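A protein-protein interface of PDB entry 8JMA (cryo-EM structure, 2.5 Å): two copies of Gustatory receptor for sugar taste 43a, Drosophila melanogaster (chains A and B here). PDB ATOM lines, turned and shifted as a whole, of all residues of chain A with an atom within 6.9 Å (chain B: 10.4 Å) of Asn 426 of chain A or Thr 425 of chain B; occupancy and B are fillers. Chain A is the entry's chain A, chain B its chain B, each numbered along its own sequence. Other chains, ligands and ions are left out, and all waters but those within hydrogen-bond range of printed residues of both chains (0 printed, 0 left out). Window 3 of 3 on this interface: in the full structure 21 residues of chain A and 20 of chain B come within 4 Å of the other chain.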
ATOM      1  N   LEU A 419     -19.698  -4.442  22.365  1.00  0.00           N
ATOM      2  CA  LEU A 419     -19.666  -4.483  23.823  1.00  0.00           C
ATOM      3  C   LEU A 419     -19.930  -5.867  24.402  1.00  0.00           C
ATOM      4  O   LEU A 419     -19.233  -6.311  25.313  1.00  0.00           O
ATOM      5  CB  LEU A 419     -20.678  -3.489  24.396  1.00  0.00           C
ATOM      6  CG  LEU A 419     -20.327  -2.012  24.212  1.00  0.00           C
ATOM      7  CD1 LEU A 419     -21.496  -1.131  24.622  1.00  0.00           C
ATOM      8  CD2 LEU A 419     -19.079  -1.657  25.006  1.00  0.00           C
ATOM      9  N   GLN A 421     -19.617  -8.821  22.868  1.00  0.00           N
ATOM     10  CA  GLN A 421     -18.598  -9.794  22.507  1.00  0.00           C
ATOM     11  C   GLN A 421     -17.374  -9.636  23.396  1.00  0.00           C
ATOM     12  O   GLN A 421     -16.813 -10.627  23.874  1.00  0.00           O
ATOM     13  CB  GLN A 421     -18.233  -9.657  21.029  1.00  0.00           C
ATOM     14  CG  GLN A 421     -17.855 -10.969  20.344  1.00  0.00           C
ATOM     15  CD  GLN A 421     -18.949 -12.013  20.390  1.00  0.00           C
ATOM     16  OE1 GLN A 421     -20.077 -11.734  20.801  1.00  0.00           O
ATOM     17  NE2 GLN A 421     -18.623 -13.227  19.961  1.00  0.00           N
ATOM     18  N   PHE A 422     -16.983  -8.393  23.681  1.00  0.00           N
ATOM     19  CA  PHE A 422     -15.848  -8.181  24.568  1.00  0.00           C
ATOM     20  C   PHE A 422     -16.113  -8.791  25.935  1.00  0.00           C
ATOM     21  O   PHE A 422     -15.221  -9.401  26.535  1.00  0.00           O
ATOM     22  CB  PHE A 422     -15.551  -6.691  24.694  1.00  0.00           C
ATOM     23  CG  PHE A 422     -14.599  -6.179  23.661  1.00  0.00           C
ATOM     24  CD1 PHE A 422     -13.282  -6.597  23.648  1.00  0.00           C
ATOM     25  CD2 PHE A 422     -15.025  -5.284  22.695  1.00  0.00           C
ATOM     26  CE1 PHE A 422     -12.410  -6.125  22.698  1.00  0.00           C
ATOM     27  CE2 PHE A 422     -14.155  -4.808  21.747  1.00  0.00           C
ATOM     28  CZ  PHE A 422     -12.851  -5.229  21.748  1.00  0.00           C
ATOM     29  N   GLN A 423     -17.337  -8.644  26.442  1.00  0.00           N
ATOM     30  CA  GLN A 423     -17.675  -9.256  27.720  1.00  0.00           C
ATOM     31  C   GLN A 423     -17.715 -10.774  27.611  1.00  0.00           C
ATOM     32  O   GLN A 423     -17.400 -11.472  28.581  1.00  0.00           O
ATOM     33  CB  GLN A 423     -19.017  -8.711  28.221  1.00  0.00           C
ATOM     34  CG  GLN A 423     -19.012  -7.224  28.579  1.00  0.00           C
ATOM     35  CD  GLN A 423     -18.020  -6.880  29.680  1.00  0.00           C
ATOM     36  OE1 GLN A 423     -17.863  -7.622  30.650  1.00  0.00           O
ATOM     37  NE2 GLN A 423     -17.329  -5.756  29.521  1.00  0.00           N
ATOM     38  N   ARG A 424     -18.080 -11.302  26.442  1.00  0.00           N
ATOM     39  CA  ARG A 424     -18.296 -12.732  26.290  1.00  0.00           C
ATOM     40  C   ARG A 424     -17.064 -13.488  25.809  1.00  0.00           C
ATOM     41  O   ARG A 424     -17.114 -14.719  25.723  1.00  0.00           O
ATOM     42  CB  ARG A 424     -19.451 -12.990  25.319  1.00  0.00           C
ATOM     43  CG  ARG A 424     -20.320 -14.169  25.714  1.00  0.00           C
ATOM     44  CD  ARG A 424     -21.037 -14.759  24.517  1.00  0.00           C
ATOM     45  NE  ARG A 424     -22.280 -15.415  24.906  1.00  0.00           N
ATOM     46  CZ  ARG A 424     -23.483 -14.862  24.838  1.00  0.00           C
ATOM     47  NH1 ARG A 424     -23.657 -13.631  24.382  1.00  0.00           N
ATOM     48  NH2 ARG A 424     -24.540 -15.561  25.239  1.00  0.00           N
ATOM     49  N   THR A 425     -15.970 -12.798  25.495  1.00  0.00           N
ATOM     50  CA  THR A 425     -14.743 -13.447  25.050  1.00  0.00           C
ATOM     51  C   THR A 425     -13.647 -13.418  26.108  1.00  0.00           C
ATOM     52  O   THR A 425     -12.485 -13.690  25.788  1.00  0.00           O
ATOM     53  CB  THR A 425     -14.230 -12.797  23.762  1.00  0.00           C
ATOM     54  OG1 THR A 425     -13.888 -11.428  24.013  1.00  0.00           O
ATOM     55  CG2 THR A 425     -15.284 -12.871  22.666  1.00  0.00           C
ATOM     56  N   ASN A 426     -13.984 -13.092  27.353  1.00  0.00           N
ATOM     57  CA  ASN A 426     -12.998 -13.032  28.427  1.00  0.00           C
ATOM     58  C   ASN A 426     -13.293 -14.073  29.503  1.00  0.00           C
ATOM     59  O   ASN A 426     -13.637 -15.215  29.200  1.00  0.00           O
ATOM     60  CB  ASN A 426     -12.969 -11.634  29.049  1.00  0.00           C
ATOM     61  CG  ASN A 426     -12.786 -10.532  28.016  1.00  0.00           C
ATOM     62  OD1 ASN A 426     -13.210  -9.397  28.232  1.00  0.00           O
ATOM     63  ND2 ASN A 426     -12.141 -10.855  26.899  1.00  0.00           N
ATOM     64  N   TYR B 312      -8.603   9.021  23.004  1.00  0.00           N
ATOM     65  CA  TYR B 312      -7.967   7.757  23.352  1.00  0.00           C
ATOM     66  C   TYR B 312      -6.835   7.962  24.352  1.00  0.00           C
ATOM     67  O   TYR B 312      -6.713   7.206  25.320  1.00  0.00           O
ATOM     68  CB  TYR B 312      -7.452   7.077  22.085  1.00  0.00           C
ATOM     69  CG  TYR B 312      -6.952   5.672  22.306  1.00  0.00           C
ATOM     70  CD1 TYR B 312      -7.772   4.703  22.866  1.00  0.00           C
ATOM     71  CD2 TYR B 312      -5.662   5.313  21.952  1.00  0.00           C
ATOM     72  CE1 TYR B 312      -7.320   3.422  23.070  1.00  0.00           C
ATOM     73  CE2 TYR B 312      -5.203   4.029  22.152  1.00  0.00           C
ATOM     74  CZ  TYR B 312      -6.038   3.088  22.710  1.00  0.00           C
ATOM     75  OH  TYR B 312      -5.588   1.805  22.912  1.00  0.00           O
ATOM     76  N   LEU B 316      -6.509   6.648  28.137  1.00  0.00           N
ATOM     77  CA  LEU B 316      -5.340   5.874  28.537  1.00  0.00           C
ATOM     78  C   LEU B 316      -4.707   6.456  29.794  1.00  0.00           C
ATOM     79  O   LEU B 316      -4.359   5.721  30.727  1.00  0.00           O
ATOM     80  CB  LEU B 316      -4.323   5.830  27.396  1.00  0.00           C
ATOM     81  CG  LEU B 316      -4.518   4.745  26.336  1.00  0.00           C
ATOM     82  CD1 LEU B 316      -3.390   4.803  25.327  1.00  0.00           C
ATOM     83  CD2 LEU B 316      -4.603   3.359  26.952  1.00  0.00           C
ATOM     84  N   LEU B 319      -6.850   5.640  32.749  1.00  0.00           N
ATOM     85  CA  LEU B 319      -6.538   4.314  33.267  1.00  0.00           C
ATOM     86  C   LEU B 319      -5.249   4.343  34.076  1.00  0.00           C
ATOM     87  O   LEU B 319      -5.172   3.750  35.159  1.00  0.00           O
ATOM     88  CB  LEU B 319      -6.426   3.308  32.122  1.00  0.00           C
ATOM     89  CG  LEU B 319      -7.685   3.030  31.297  1.00  0.00           C
ATOM     90  CD1 LEU B 319      -7.625   1.624  30.731  1.00  0.00           C
ATOM     91  CD2 LEU B 319      -8.962   3.232  32.103  1.00  0.00           C
ATOM     92  N   VAL B 417     -15.420   3.362  21.084  1.00  0.00           N
ATOM     93  CA  VAL B 417     -15.924   2.171  21.752  1.00  0.00           C
ATOM     94  C   VAL B 417     -15.031   0.963  21.495  1.00  0.00           C
ATOM     95  O   VAL B 417     -14.719   0.210  22.415  1.00  0.00           O
ATOM     96  CB  VAL B 417     -17.351   1.828  21.286  1.00  0.00           C
ATOM     97  CG1 VAL B 417     -17.727   0.418  21.713  1.00  0.00           C
ATOM     98  CG2 VAL B 417     -18.348   2.840  21.829  1.00  0.00           C
ATOM     99  N   ILE B 418     -14.621   0.779  20.244  1.00  0.00           N
ATOM    100  CA  ILE B 418     -13.760  -0.345  19.900  1.00  0.00           C
ATOM    101  C   ILE B 418     -12.384  -0.253  20.551  1.00  0.00           C
ATOM    102  O   ILE B 418     -11.882  -1.234  21.099  1.00  0.00           O
ATOM    103  CB  ILE B 418     -13.558  -0.440  18.377  1.00  0.00           C
ATOM    104  CG1 ILE B 418     -14.896  -0.680  17.674  1.00  0.00           C
ATOM    105  CG2 ILE B 418     -12.580  -1.554  18.042  1.00  0.00           C
ATOM    106  CD1 ILE B 418     -14.800  -0.660  16.164  1.00  0.00           C
ATOM    107  N   LEU B 419     -11.778   0.929  20.490  1.00  0.00           N
ATOM    108  CA  LEU B 419     -10.453   1.135  21.066  1.00  0.00           C
ATOM    109  C   LEU B 419     -10.425   1.018  22.584  1.00  0.00           C
ATOM    110  O   LEU B 419      -9.540   0.378  23.151  1.00  0.00           O
ATOM    111  CB  LEU B 419      -9.911   2.504  20.653  1.00  0.00           C
ATOM    112  CG  LEU B 419      -9.525   2.632  19.180  1.00  0.00           C
ATOM    113  CD1 LEU B 419      -9.206   4.077  18.832  1.00  0.00           C
ATOM    114  CD2 LEU B 419      -8.348   1.724  18.865  1.00  0.00           C
ATOM    115  N   ILE B 420     -11.400   1.640  23.238  1.00  0.00           N
ATOM    116  CA  ILE B 420     -11.477   1.606  24.692  1.00  0.00           C
ATOM    117  C   ILE B 420     -11.750   0.210  25.224  1.00  0.00           C
ATOM    118  O   ILE B 420     -11.161  -0.205  26.222  1.00  0.00           O
ATOM    119  CB  ILE B 420     -12.557   2.560  25.231  1.00  0.00           C
ATOM    120  CG1 ILE B 420     -12.101   4.012  25.083  1.00  0.00           C
ATOM    121  CG2 ILE B 420     -12.852   2.255  26.691  1.00  0.00           C
ATOM    122  CD1 ILE B 420     -13.199   5.023  25.333  1.00  0.00           C
ATOM    123  N   GLN B 421     -12.641  -0.519  24.561  1.00  0.00           N
ATOM    124  CA  GLN B 421     -12.979  -1.851  25.040  1.00  0.00           C
ATOM    125  C   GLN B 421     -11.774  -2.772  24.940  1.00  0.00           C
ATOM    126  O   GLN B 421     -11.487  -3.535  25.869  1.00  0.00           O
ATOM    127  CB  GLN B 421     -14.172  -2.407  24.265  1.00  0.00           C
ATOM    128  CG  GLN B 421     -15.091  -3.315  25.079  1.00  0.00           C
ATOM    129  CD  GLN B 421     -15.687  -2.639  26.296  1.00  0.00           C
ATOM    130  OE1 GLN B 421     -15.551  -1.429  26.480  1.00  0.00           O
ATOM    131  NE2 GLN B 421     -16.359  -3.421  27.133  1.00  0.00           N
ATOM    132  N   PHE B 422     -11.018  -2.671  23.846  1.00  0.00           N
ATOM    133  CA  PHE B 422      -9.822  -3.494  23.719  1.00  0.00           C
ATOM    134  C   PHE B 422      -8.850  -3.206  24.850  1.00  0.00           C
ATOM    135  O   PHE B 422      -8.239  -4.126  25.403  1.00  0.00           O
ATOM    136  CB  PHE B 422      -9.161  -3.252  22.366  1.00  0.00           C
ATOM    137  CG  PHE B 422      -9.666  -4.149  21.282  1.00  0.00           C
ATOM    138  CD1 PHE B 422      -9.431  -5.510  21.327  1.00  0.00           C
ATOM    139  CD2 PHE B 422     -10.387  -3.631  20.220  1.00  0.00           C
ATOM    140  CE1 PHE B 422      -9.896  -6.332  20.330  1.00  0.00           C
ATOM    141  CE2 PHE B 422     -10.849  -4.449  19.220  1.00  0.00           C
ATOM    142  CZ  PHE B 422     -10.606  -5.797  19.276  1.00  0.00           C
ATOM    143  N   GLN B 423      -8.694  -1.932  25.212  1.00  0.00           N
ATOM    144  CA  GLN B 423      -7.823  -1.592  26.329  1.00  0.00           C
ATOM    145  C   GLN B 423      -8.403  -2.078  27.648  1.00  0.00           C
ATOM    146  O   GLN B 423      -7.651  -2.427  28.565  1.00  0.00           O
ATOM    147  CB  GLN B 423      -7.583  -0.079  26.363  1.00  0.00           C
ATOM    148  CG  GLN B 423      -6.797   0.473  25.174  1.00  0.00           C
ATOM    149  CD  GLN B 423      -5.407  -0.135  25.045  1.00  0.00           C
ATOM    150  OE1 GLN B 423      -4.713  -0.352  26.039  1.00  0.00           O
ATOM    151  NE2 GLN B 423      -5.004  -0.430  23.814  1.00  0.00           N
ATOM    152  N   ARG B 424      -9.732  -2.124  27.762  1.00  0.00           N
ATOM    153  CA  ARG B 424     -10.375  -2.425  29.032  1.00  0.00           C
ATOM    154  C   ARG B 424     -10.693  -3.903  29.219  1.00  0.00           C
ATOM    155  O   ARG B 424     -11.166  -4.281  30.296  1.00  0.00           O
ATOM    156  CB  ARG B 424     -11.666  -1.615  29.173  1.00  0.00           C
ATOM    157  CG  ARG B 424     -11.922  -1.130  30.587  1.00  0.00           C
ATOM    158  CD  ARG B 424     -13.395  -0.876  30.831  1.00  0.00           C
ATOM    159  NE  ARG B 424     -13.602   0.127  31.869  1.00  0.00           N
ATOM    160  CZ  ARG B 424     -13.836   1.413  31.644  1.00  0.00           C
ATOM    161  NH1 ARG B 424     -13.919   1.901  30.416  1.00  0.00           N
ATOM    162  NH2 ARG B 424     -13.993   2.233  32.679  1.00  0.00           N
ATOM    163  N   THR B 425     -10.450  -4.745  28.216  1.00  0.00           N
ATOM    164  CA  THR B 425     -10.702  -6.176  28.325  1.00  0.00           C
ATOM    165  C   THR B 425      -9.421  -6.992  28.434  1.00  0.00           C
ATOM    166  O   THR B 425      -9.463  -8.215  28.270  1.00  0.00           O
ATOM    167  CB  THR B 425     -11.522  -6.666  27.127  1.00  0.00           C
ATOM    168  OG1 THR B 425     -10.772  -6.485  25.919  1.00  0.00           O
ATOM    169  CG2 THR B 425     -12.840  -5.911  27.032  1.00  0.00           C
ATOM    170  N   ASN B 426      -8.288  -6.349  28.703  1.00  0.00           N
ATOM    171  CA  ASN B 426      -7.013  -7.050  28.818  1.00  0.00           C
ATOM    172  C   ASN B 426      -6.446  -6.928  30.229  1.00  0.00           C
ATOM    173  O   ASN B 426      -7.172  -7.044  31.214  1.00  0.00           O
ATOM    174  CB  ASN B 426      -6.008  -6.501  27.803  1.00  0.00           C
ATOM    175  CG  ASN B 426      -6.550  -6.491  26.381  1.00  0.00           C
ATOM    176  OD1 ASN B 426      -6.124  -5.684  25.556  1.00  0.00           O
ATOM    177  ND2 ASN B 426      -7.478  -7.396  26.084  1.00  0.00           N
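The side-chain amide nitrogen of Gln 423 of chain A sits close to the side-chain amide nitrogen of Gln 421 of chain B (3.5 Å).
The backbone carbonyl oxygen (O) of Phe 422 of chain A sits close to the side-chain amide oxygen (OD1) of Asn 426 of chain A (2.6 Å). ND2 of Asn 426 of chain A sits close to OG1 of Thr 425 of chain A, at 3.4 Å. The backbone carbonyl oxygen (O) of Gln 421 of chain B sits close to the side-chain hydroxyl (OG1) of Thr 425 of chain B (3.0 Å). The backbone carbonyl oxygen (O) of Phe 422 of chain B sits at hydrogen-bond distance from the side-chain hydroxyl (OG1) of Thr 425 of chain B, 3.5 Å away. The side-chain amide oxygen (OD1) of Asn 426 of chain B sits close to the backbone carbonyl oxygen (O) of Phe 422 of chain B (2.6 Å). The side-chain hydroxyl of Thr 425 of chain B sits close to the side-chain amide nitrogen of Asn 426 of chain B, 3.4 Å away.
Among the printed residues, pairs that only touch across the chains: Phe 422 of chain A with Gln 421 of chain B (3.1 Å), Phe 422 of chain A with Phe 422 of chain B (3.3 Å), Phe 422 of chain A with Thr 425 of chain B (3.4 Å), Asn 426 of chain A with Thr 425 of chain B (3.4 Å) and Leu 419 of chain A with Gln 421 of chain B (3.8 Å).
Of the printed residues of chain B, Leu 419 of chain A touches Gln 421. Of chain B, only Gln 421, Phe 422 and Thr 425 come within 4 Å of Phe 422 of chain A. Gln 423 of chain A touches one residue of chain B. Arg 424 of chain A touches none of the printed residues of chain B. No residue of chain B comes within 4 Å of Thr 425 of chain A. Of the printed residues of chain A, Gln 421 of chain B touches Leu 419 (3.8 Å), Phe 422 (3.1 Å) and Gln 423 (3.5 Å). Of the printed residues of chain A, Phe 422 of chain B touches Phe 422 (3.3 Å). Of chain A, only Phe 422 (3.4 Å) and Asn 426 (3.4 Å) come within 4 Å of Thr 425 of chain B. The nearest printed residue of chain B that does not touch Leu 419 of chain A is Val 417 of chain B (4.1 Å).
Of the 13 printed residues of chain B, 3 touch a printed residue of chain A. Hydrophobic or aromatic side chains of chain B within 4 Å of the printed part of chain A: Phe 422. Of the 7 printed residues of chain A, 4 touch a printed residue of chain B. Hydrophobic or aromatic side chains of chain A within 4 Å of the printed part of chain B: Leu 419 and Phe 422. Among the printed residues, 6 pairs touch across the chains. Among the printed residues, no Asp or Glu carboxylate lies within 4 Å of a Lys or Arg side-chain nitrogen of the other chain.
Leu 419 of chain A touches Gln 421 of chain B, but with the chains exchanged Gln 421 of chain A does not touch Leu 419 of chain B (12.3 Å). Phe 422 of chain A touches Gln 421 of chain B, but with the chains exchanged Gln 421 of chain A does not touch Phe 422 of chain B (8.7 Å). Phe 422 of chain A touches Thr 425 of chain B, but with the chains exchanged Thr 425 of chain A does not touch Phe 422 of chain B (7.4 Å). Gln 423 of chain A touches Gln 421 of chain B, but with the chains exchanged Gln 421 of chain A does not touch Gln 423 of chain B (11.7 Å). Positions printed for both chains: 419, 421, 422, 423, 424, 425 and 426. Of the 6 pairs that touch across the chains among the printed residues, 1 has its exchanged pair printed and touching as well.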
